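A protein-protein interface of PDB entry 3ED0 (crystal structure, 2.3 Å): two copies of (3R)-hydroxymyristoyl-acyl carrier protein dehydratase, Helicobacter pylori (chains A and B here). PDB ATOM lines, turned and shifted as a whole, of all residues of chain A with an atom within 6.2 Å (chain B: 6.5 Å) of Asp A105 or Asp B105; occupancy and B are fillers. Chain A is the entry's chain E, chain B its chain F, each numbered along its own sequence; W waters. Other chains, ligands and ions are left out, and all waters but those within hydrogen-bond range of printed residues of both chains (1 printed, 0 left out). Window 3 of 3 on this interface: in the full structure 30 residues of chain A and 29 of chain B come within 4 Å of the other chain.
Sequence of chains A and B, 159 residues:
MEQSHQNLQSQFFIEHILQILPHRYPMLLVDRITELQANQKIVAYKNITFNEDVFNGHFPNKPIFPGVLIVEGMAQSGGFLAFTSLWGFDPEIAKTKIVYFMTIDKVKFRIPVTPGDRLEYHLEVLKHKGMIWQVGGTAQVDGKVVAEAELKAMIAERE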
ATOM      1  N   THR A 103     -21.980 -16.701   0.316  1.00  0.00           N
ATOM      2  CA  THR A 103     -22.068 -18.121   0.650  1.00  0.00           C
ATOM      3  C   THR A 103     -23.448 -18.690   0.321  1.00  0.00           C
ATOM      4  O   THR A 103     -24.433 -17.958   0.187  1.00  0.00           O
ATOM      5  CB  THR A 103     -21.786 -18.392   2.162  1.00  0.00           C
ATOM      6  OG1 THR A 103     -22.788 -17.757   2.959  1.00  0.00           O
ATOM      7  CG2 THR A 103     -20.423 -17.865   2.572  1.00  0.00           C
ATOM      8  N   ILE A 104     -23.498 -20.009   0.191  1.00  0.00           N
ATOM      9  CA  ILE A 104     -24.732 -20.724  -0.098  1.00  0.00           C
ATOM     10  C   ILE A 104     -24.682 -21.977   0.761  1.00  0.00           C
ATOM     11  O   ILE A 104     -23.660 -22.655   0.799  1.00  0.00           O
ATOM     12  CB  ILE A 104     -24.815 -21.145  -1.585  1.00  0.00           C
ATOM     13  CG1 ILE A 104     -24.714 -19.918  -2.489  1.00  0.00           C
ATOM     14  CG2 ILE A 104     -26.121 -21.881  -1.846  1.00  0.00           C
ATOM     15  CD1 ILE A 104     -24.703 -20.251  -3.958  1.00  0.00           C
ATOM     16  N   ASP A 105     -25.771 -22.277   1.459  1.00  0.00           N
ATOM     17  CA  ASP A 105     -25.800 -23.467   2.299  1.00  0.00           C
ATOM     18  C   ASP A 105     -27.147 -24.144   2.389  1.00  0.00           C
ATOM     19  O   ASP A 105     -28.191 -23.561   2.075  1.00  0.00           O
ATOM     20  CB  ASP A 105     -25.357 -23.151   3.727  1.00  0.00           C
ATOM     21  CG  ASP A 105     -23.944 -22.653   3.804  1.00  0.00           C
ATOM     22  OD1 ASP A 105     -23.751 -21.417   3.886  1.00  0.00           O
ATOM     23  OD2 ASP A 105     -23.024 -23.497   3.774  1.00  0.00           O
ATOM     24  N   LYS A 106     -27.096 -25.393   2.832  1.00  0.00           N
ATOM     25  CA  LYS A 106     -28.281 -26.195   3.050  1.00  0.00           C
ATOM     26  C   LYS A 106     -29.347 -26.057   1.976  1.00  0.00           C
ATOM     27  O   LYS A 106     -30.526 -25.906   2.297  1.00  0.00           O
ATOM     28  CB  LYS A 106     -28.893 -25.835   4.418  1.00  0.00           C
ATOM     29  CG  LYS A 106     -27.895 -25.826   5.582  1.00  0.00           C
ATOM     30  CD  LYS A 106     -28.604 -25.595   6.926  1.00  0.00           C
ATOM     31  CE  LYS A 106     -27.612 -25.413   8.096  1.00  0.00           C
ATOM     32  NZ  LYS A 106     -26.917 -24.078   8.062  1.00  0.00           N
ATOM     33  N   VAL A 107     -28.965 -26.072   0.705  1.00  0.00           N
ATOM     34  CA  VAL A 107     -29.999 -25.987  -0.318  1.00  0.00           C
ATOM     35  C   VAL A 107     -30.366 -27.417  -0.692  1.00  0.00           C
ATOM     36  O   VAL A 107     -29.506 -28.299  -0.763  1.00  0.00           O
ATOM     37  CB  VAL A 107     -29.556 -25.185  -1.580  1.00  0.00           C
ATOM     38  CG1 VAL A 107     -28.310 -24.399  -1.286  1.00  0.00           C
ATOM     39  CG2 VAL A 107     -29.388 -26.100  -2.766  1.00  0.00           C
ATOM     40  N   LYS A 108     -31.653 -27.642  -0.904  1.00  0.00           N
ATOM     41  CA  LYS A 108     -32.167 -28.960  -1.252  1.00  0.00           C
ATOM     42  C   LYS A 108     -33.250 -28.770  -2.311  1.00  0.00           C
ATOM     43  O   LYS A 108     -34.147 -27.947  -2.137  1.00  0.00           O
ATOM     44  CB  LYS A 108     -32.758 -29.620   0.010  1.00  0.00           C
ATOM     45  CG  LYS A 108     -33.173 -31.080  -0.133  1.00  0.00           C
ATOM     46  CD  LYS A 108     -33.699 -31.650   1.195  1.00  0.00           C
ATOM     47  CE  LYS A 108     -34.240 -33.078   1.017  1.00  0.00           C
ATOM     48  NZ  LYS A 108     -34.819 -33.678   2.282  1.00  0.00           N
ATOM     49  N   GLN A 134     -27.951 -12.110   5.425  1.00  0.00           N
ATOM     50  CA  GLN A 134     -28.030 -13.561   5.435  1.00  0.00           C
ATOM     51  C   GLN A 134     -29.499 -13.945   5.473  1.00  0.00           C
ATOM     52  O   GLN A 134     -30.173 -13.786   6.498  1.00  0.00           O
ATOM     53  CB  GLN A 134     -27.292 -14.127   6.649  1.00  0.00           C
ATOM     54  CG  GLN A 134     -27.604 -15.591   6.925  1.00  0.00           C
ATOM     55  CD  GLN A 134     -26.363 -16.425   7.173  1.00  0.00           C
ATOM     56  OE1 GLN A 134     -25.553 -16.111   8.052  1.00  0.00           O
ATOM     57  NE2 GLN A 134     -26.206 -17.496   6.398  1.00  0.00           N
ATOM     58  N   GLU A 148     -35.306 -25.446  -1.016  1.00  0.00           N
ATOM     59  CA  GLU A 148     -34.942 -24.843   0.260  1.00  0.00           C
ATOM     60  C   GLU A 148     -33.555 -24.259   0.080  1.00  0.00           C
ATOM     61  O   GLU A 148     -32.731 -24.833  -0.632  1.00  0.00           O
ATOM     62  CB  GLU A 148     -34.885 -25.904   1.362  1.00  0.00           C
ATOM     63  CG  GLU A 148     -36.176 -26.649   1.585  1.00  0.00           C
ATOM     64  CD  GLU A 148     -35.974 -27.908   2.398  1.00  0.00           C
ATOM     65  OE1 GLU A 148     -36.955 -28.651   2.588  1.00  0.00           O
ATOM     66  OE2 GLU A 148     -34.838 -28.157   2.849  1.00  0.00           O
ATOM     67  N   ALA A 149     -33.283 -23.131   0.721  1.00  0.00           N
ATOM     68  CA  ALA A 149     -31.967 -22.526   0.591  1.00  0.00           C
ATOM     69  C   ALA A 149     -31.628 -21.450   1.613  1.00  0.00           C
ATOM     70  O   ALA A 149     -32.493 -20.711   2.095  1.00  0.00           O
ATOM     71  CB  ALA A 149     -31.802 -21.962  -0.800  1.00  0.00           C
ATOM     72  N   GLU A 150     -30.340 -21.375   1.923  1.00  0.00           N
ATOM     73  CA  GLU A 150     -29.804 -20.393   2.845  1.00  0.00           C
ATOM     74  C   GLU A 150     -28.651 -19.729   2.105  1.00  0.00           C
ATOM     75  O   GLU A 150     -27.821 -20.415   1.502  1.00  0.00           O
ATOM     76  CB  GLU A 150     -29.280 -21.084   4.097  1.00  0.00           C
ATOM     77  CG  GLU A 150     -28.617 -20.152   5.081  1.00  0.00           C
ATOM     78  CD  GLU A 150     -28.046 -20.906   6.256  1.00  0.00           C
ATOM     79  OE1 GLU A 150     -28.807 -21.685   6.876  1.00  0.00           O
ATOM     80  OE2 GLU A 150     -26.839 -20.719   6.551  1.00  0.00           O
ATOM     81  N   LEU A 151     -28.587 -18.402   2.149  1.00  0.00           N
ATOM     82  CA  LEU A 151     -27.521 -17.695   1.454  1.00  0.00           C
ATOM     83  C   LEU A 151     -27.186 -16.360   2.091  1.00  0.00           C
ATOM     84  O   LEU A 151     -28.014 -15.741   2.757  1.00  0.00           O
ATOM     85  CB  LEU A 151     -27.912 -17.476  -0.013  1.00  0.00           C
ATOM     86  CG  LEU A 151     -29.002 -16.433  -0.265  1.00  0.00           C
ATOM     87  CD1 LEU A 151     -28.337 -15.100  -0.615  1.00  0.00           C
ATOM     88  CD2 LEU A 151     -29.919 -16.888  -1.400  1.00  0.00           C
ATOM     89  N   THR B 103     -28.688 -31.472  -3.799  1.00  0.00           N
ATOM     90  CA  THR B 103     -28.326 -30.582  -2.697  1.00  0.00           C
ATOM     91  C   THR B 103     -27.061 -29.789  -3.007  1.00  0.00           C
ATOM     92  O   THR B 103     -26.244 -30.185  -3.839  1.00  0.00           O
ATOM     93  CB  THR B 103     -28.086 -31.344  -1.357  1.00  0.00           C
ATOM     94  OG1 THR B 103     -26.962 -32.225  -1.489  1.00  0.00           O
ATOM     95  CG2 THR B 103     -29.327 -32.141  -0.965  1.00  0.00           C
ATOM     96  N   ILE B 104     -26.926 -28.654  -2.336  1.00  0.00           N
ATOM     97  CA  ILE B 104     -25.766 -27.789  -2.480  1.00  0.00           C
ATOM     98  C   ILE B 104     -25.444 -27.351  -1.059  1.00  0.00           C
ATOM     99  O   ILE B 104     -26.345 -27.020  -0.298  1.00  0.00           O
ATOM    100  CB  ILE B 104     -26.074 -26.521  -3.315  1.00  0.00           C
ATOM    101  CG1 ILE B 104     -26.602 -26.903  -4.699  1.00  0.00           C
ATOM    102  CG2 ILE B 104     -24.814 -25.684  -3.454  1.00  0.00           C
ATOM    103  CD1 ILE B 104     -27.020 -25.700  -5.545  1.00  0.00           C
ATOM    104  N   ASP B 105     -24.170 -27.353  -0.691  1.00  0.00           N
ATOM    105  CA  ASP B 105     -23.830 -26.940   0.655  1.00  0.00           C
ATOM    106  C   ASP B 105     -22.394 -26.467   0.817  1.00  0.00           C
ATOM    107  O   ASP B 105     -21.520 -26.776   0.005  1.00  0.00           O
ATOM    108  CB  ASP B 105     -24.127 -28.076   1.642  1.00  0.00           C
ATOM    109  CG  ASP B 105     -24.224 -27.588   3.080  1.00  0.00           C
ATOM    110  OD1 ASP B 105     -24.534 -26.387   3.291  1.00  0.00           O
ATOM    111  OD2 ASP B 105     -24.002 -28.403   4.001  1.00  0.00           O
ATOM    112  N   LYS B 106     -22.177 -25.692   1.873  1.00  0.00           N
ATOM    113  CA  LYS B 106     -20.867 -25.160   2.199  1.00  0.00           C
ATOM    114  C   LYS B 106     -20.163 -24.483   1.026  1.00  0.00           C
ATOM    115  O   LYS B 106     -18.987 -24.748   0.764  1.00  0.00           O
ATOM    116  CB  LYS B 106     -19.987 -26.277   2.763  1.00  0.00           C
ATOM    117  CG  LYS B 106     -20.608 -26.999   3.952  1.00  0.00           C
ATOM    118  CD  LYS B 106     -19.646 -28.017   4.542  1.00  0.00           C
ATOM    119  CE  LYS B 106     -20.308 -28.858   5.634  1.00  0.00           C
ATOM    120  NZ  LYS B 106     -21.293 -29.827   5.047  1.00  0.00           N
ATOM    121  N   VAL B 107     -20.875 -23.624   0.305  1.00  0.00           N
ATOM    122  CA  VAL B 107     -20.230 -22.932  -0.798  1.00  0.00           C
ATOM    123  C   VAL B 107     -19.849 -21.529  -0.334  1.00  0.00           C
ATOM    124  O   VAL B 107     -20.602 -20.860   0.381  1.00  0.00           O
ATOM    125  CB  VAL B 107     -21.115 -22.872  -2.102  1.00  0.00           C
ATOM    126  CG1 VAL B 107     -22.381 -23.669  -1.921  1.00  0.00           C
ATOM    127  CG2 VAL B 107     -21.409 -21.444  -2.494  1.00  0.00           C
ATOM    128  N   LYS B 108     -18.654 -21.111  -0.727  1.00  0.00           N
ATOM    129  CA  LYS B 108     -18.144 -19.807  -0.364  1.00  0.00           C
ATOM    130  C   LYS B 108     -17.411 -19.245  -1.560  1.00  0.00           C
ATOM    131  O   LYS B 108     -16.629 -19.950  -2.203  1.00  0.00           O
ATOM    132  CB  LYS B 108     -17.196 -19.944   0.828  1.00  0.00           C
ATOM    133  CG  LYS B 108     -17.780 -20.827   1.918  1.00  0.00           C
ATOM    134  CD  LYS B 108     -16.819 -21.079   3.068  1.00  0.00           C
ATOM    135  CE  LYS B 108     -17.417 -22.108   4.041  1.00  0.00           C
ATOM    136  NZ  LYS B 108     -16.580 -22.255   5.280  1.00  0.00           N
ATOM    137  N   GLU B 148     -15.505 -22.517  -3.210  1.00  0.00           N
ATOM    138  CA  GLU B 148     -15.523 -23.868  -2.657  1.00  0.00           C
ATOM    139  C   GLU B 148     -16.975 -24.304  -2.665  1.00  0.00           C
ATOM    140  O   GLU B 148     -17.876 -23.468  -2.569  1.00  0.00           O
ATOM    141  CB  GLU B 148     -15.044 -23.867  -1.213  1.00  0.00           C
ATOM    142  CG  GLU B 148     -13.853 -22.992  -0.969  1.00  0.00           C
ATOM    143  CD  GLU B 148     -13.668 -22.684   0.499  1.00  0.00           C
ATOM    144  OE1 GLU B 148     -12.847 -21.789   0.801  1.00  0.00           O
ATOM    145  OE2 GLU B 148     -14.339 -23.333   1.339  1.00  0.00           O
ATOM    146  N   ALA B 149     -17.211 -25.606  -2.764  1.00  0.00           N
ATOM    147  CA  ALA B 149     -18.579 -26.092  -2.769  1.00  0.00           C
ATOM    148  C   ALA B 149     -18.686 -27.602  -2.668  1.00  0.00           C
ATOM    149  O   ALA B 149     -17.778 -28.333  -3.067  1.00  0.00           O
ATOM    150  CB  ALA B 149     -19.288 -25.612  -4.030  1.00  0.00           C
ATOM    151  N   GLU B 150     -19.794 -28.056  -2.094  1.00  0.00           N
ATOM    152  CA  GLU B 150     -20.085 -29.480  -1.993  1.00  0.00           C
ATOM    153  C   GLU B 150     -21.458 -29.599  -2.638  1.00  0.00           C
ATOM    154  O   GLU B 150     -22.260 -28.665  -2.573  1.00  0.00           O
ATOM    155  CB  GLU B 150     -20.167 -29.960  -0.538  1.00  0.00           C
ATOM    156  CG  GLU B 150     -18.876 -29.854   0.259  1.00  0.00           C
ATOM    157  CD  GLU B 150     -18.920 -30.672   1.544  1.00  0.00           C
ATOM    158  OE1 GLU B 150     -20.009 -30.788   2.146  1.00  0.00           O
ATOM    159  OE2 GLU B 150     -17.860 -31.195   1.957  1.00  0.00           O
ATOM    160  N   LEU B 151     -21.733 -30.732  -3.265  1.00  0.00           N
ATOM    161  CA  LEU B 151     -23.023 -30.900  -3.907  1.00  0.00           C
ATOM    162  C   LEU B 151     -23.328 -32.360  -4.193  1.00  0.00           C
ATOM    163  O   LEU B 151     -22.433 -33.206  -4.235  1.00  0.00           O
ATOM    164  CB  LEU B 151     -23.069 -30.075  -5.202  1.00  0.00           C
ATOM    165  CG  LEU B 151     -22.133 -30.504  -6.333  1.00  0.00           C
ATOM    166  CD1 LEU B 151     -22.866 -31.492  -7.231  1.00  0.00           C
ATOM    167  CD2 LEU B 151     -21.701 -29.294  -7.141  1.00  0.00           C
ATOM    168  N   LYS B 152     -24.613 -32.639  -4.381  1.00  0.00           N
ATOM    169  CA  LYS B 152     -25.092 -33.981  -4.663  1.00  0.00           C
ATOM    170  C   LYS B 152     -26.073 -33.895  -5.835  1.00  0.00           C
ATOM    171  O   LYS B 152     -26.971 -33.044  -5.854  1.00  0.00           O
ATOM    172  CB  LYS B 152     -25.780 -34.547  -3.420  1.00  0.00           C
ATOM    173  CG  LYS B 152     -26.161 -36.009  -3.522  1.00  0.00           C
ATOM    174  CD  LYS B 152     -26.653 -36.544  -2.179  1.00  0.00           C
ATOM    175  CE  LYS B 152     -27.945 -35.863  -1.726  1.00  0.00           C
ATOM    176  NZ  LYS B 152     -28.422 -36.377  -0.406  1.00  0.00           N
HETATM  177  O   HOH W   1     -20.768 -22.010   3.211  1.00  0.00           O
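Among the printed residues, merely in contact across the chains: Thr A103 with Val B107, Ile A104 with Lys B106, Lys A106 with Ile B104 and Val A107 with Thr B103.
Of the printed residues of chain B, Asp A105 touches Asp B105 (3.3 Å) and Lys B106 (3.0 Å). Printed residues of chain A within 4 Å of Asp B105: Asp A105 and Lys A106. Of the printed residues of chain A, Val B107 touches Thr A103 (3.1 Å) and Ile A104 (3.0 Å). Of the printed residues of chain A, Lys B106 touches Ile A104 and Asp A105. Printed residues of chain B within 4 Å of Lys A106: Ile B104 (3.6 Å) and Asp B105 (2.8 Å). Printed residues of chain B within 4 Å of Val A107: Thr B103 (3.2 Å) and Ile B104 (3.0 Å). Of the printed residues of chain A, Ile B104 touches Lys A106 (3.6 Å) and Val A107 (3.0 Å). The nearest printed residue of chain B that does not touch Asp A105 is Ile B104 (4.02 Å). The nearest printed residue of chain B that does not touch Lys A106 is Lys B106 (5.0 Å).
Thr A103 touches Val B107, and with the chains exchanged Val A107 touches Thr B103. Ile A104 touches Lys B106, and with the chains exchanged Lys A106 touches Ile B104. Ile A104 touches Val B107, and with the chains exchanged Val A107 touches Ile B104. Asp B105 touches its own counterpart, Asp A105.
NZ of Lys B106 lies within salt-bridge range of OD2 of Asp B105 (3.2 Å). The side-chain carboxylate of Glu A150 lies within salt-bridge range of the side-chain amino group of Lys A106. O of Thr B103 lies within hydrogen-bond range of N of Lys B152, at 3.0 Å. The backbone NH (N) of Asp B105 lies within hydrogen-bond range of the backbone carbonyl oxygen (O) of Glu B150. The backbone NH (N) of Asp A105 is in hydrogen-bond range of the backbone carbonyl oxygen (O) of Glu A150 (2.8 Å). NZ of Lys B106 is in salt-bridge range of OE1 of Glu B150, 3.3 Å away.
Of the 11 printed residues of chain A, 5 touch a printed residue of chain B. Hydrophobic or aromatic side chains of chain A within 4 Å of the printed part of chain B: Ile A104 and Val A107. Among the printed residues, 9 pairs touch across the chains.
N of Lys B106 is in hydrogen-bond range of OD2 of Asp A105. O of Ile A104 lies within hydrogen-bond range of N of Val B107, at 3.0 Å. The side-chain carboxylate of Asp A105 sits close to the side-chain carboxylate of Asp B105 (3.3 Å). The backbone carbonyl oxygen (O) of Ile B104 lies within hydrogen-bond range of the backbone NH (N) of Val A107 (3.0 Å). The side-chain carboxylate (OD1) of Asp B105 sits at hydrogen-bond distance from the backbone NH (N) of Lys A106 (2.8 Å).
Water W1 lies within hydrogen-bond range of OD2 of Asp A105 (2.8 Å) and O of Val B107 (3.1 Å).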
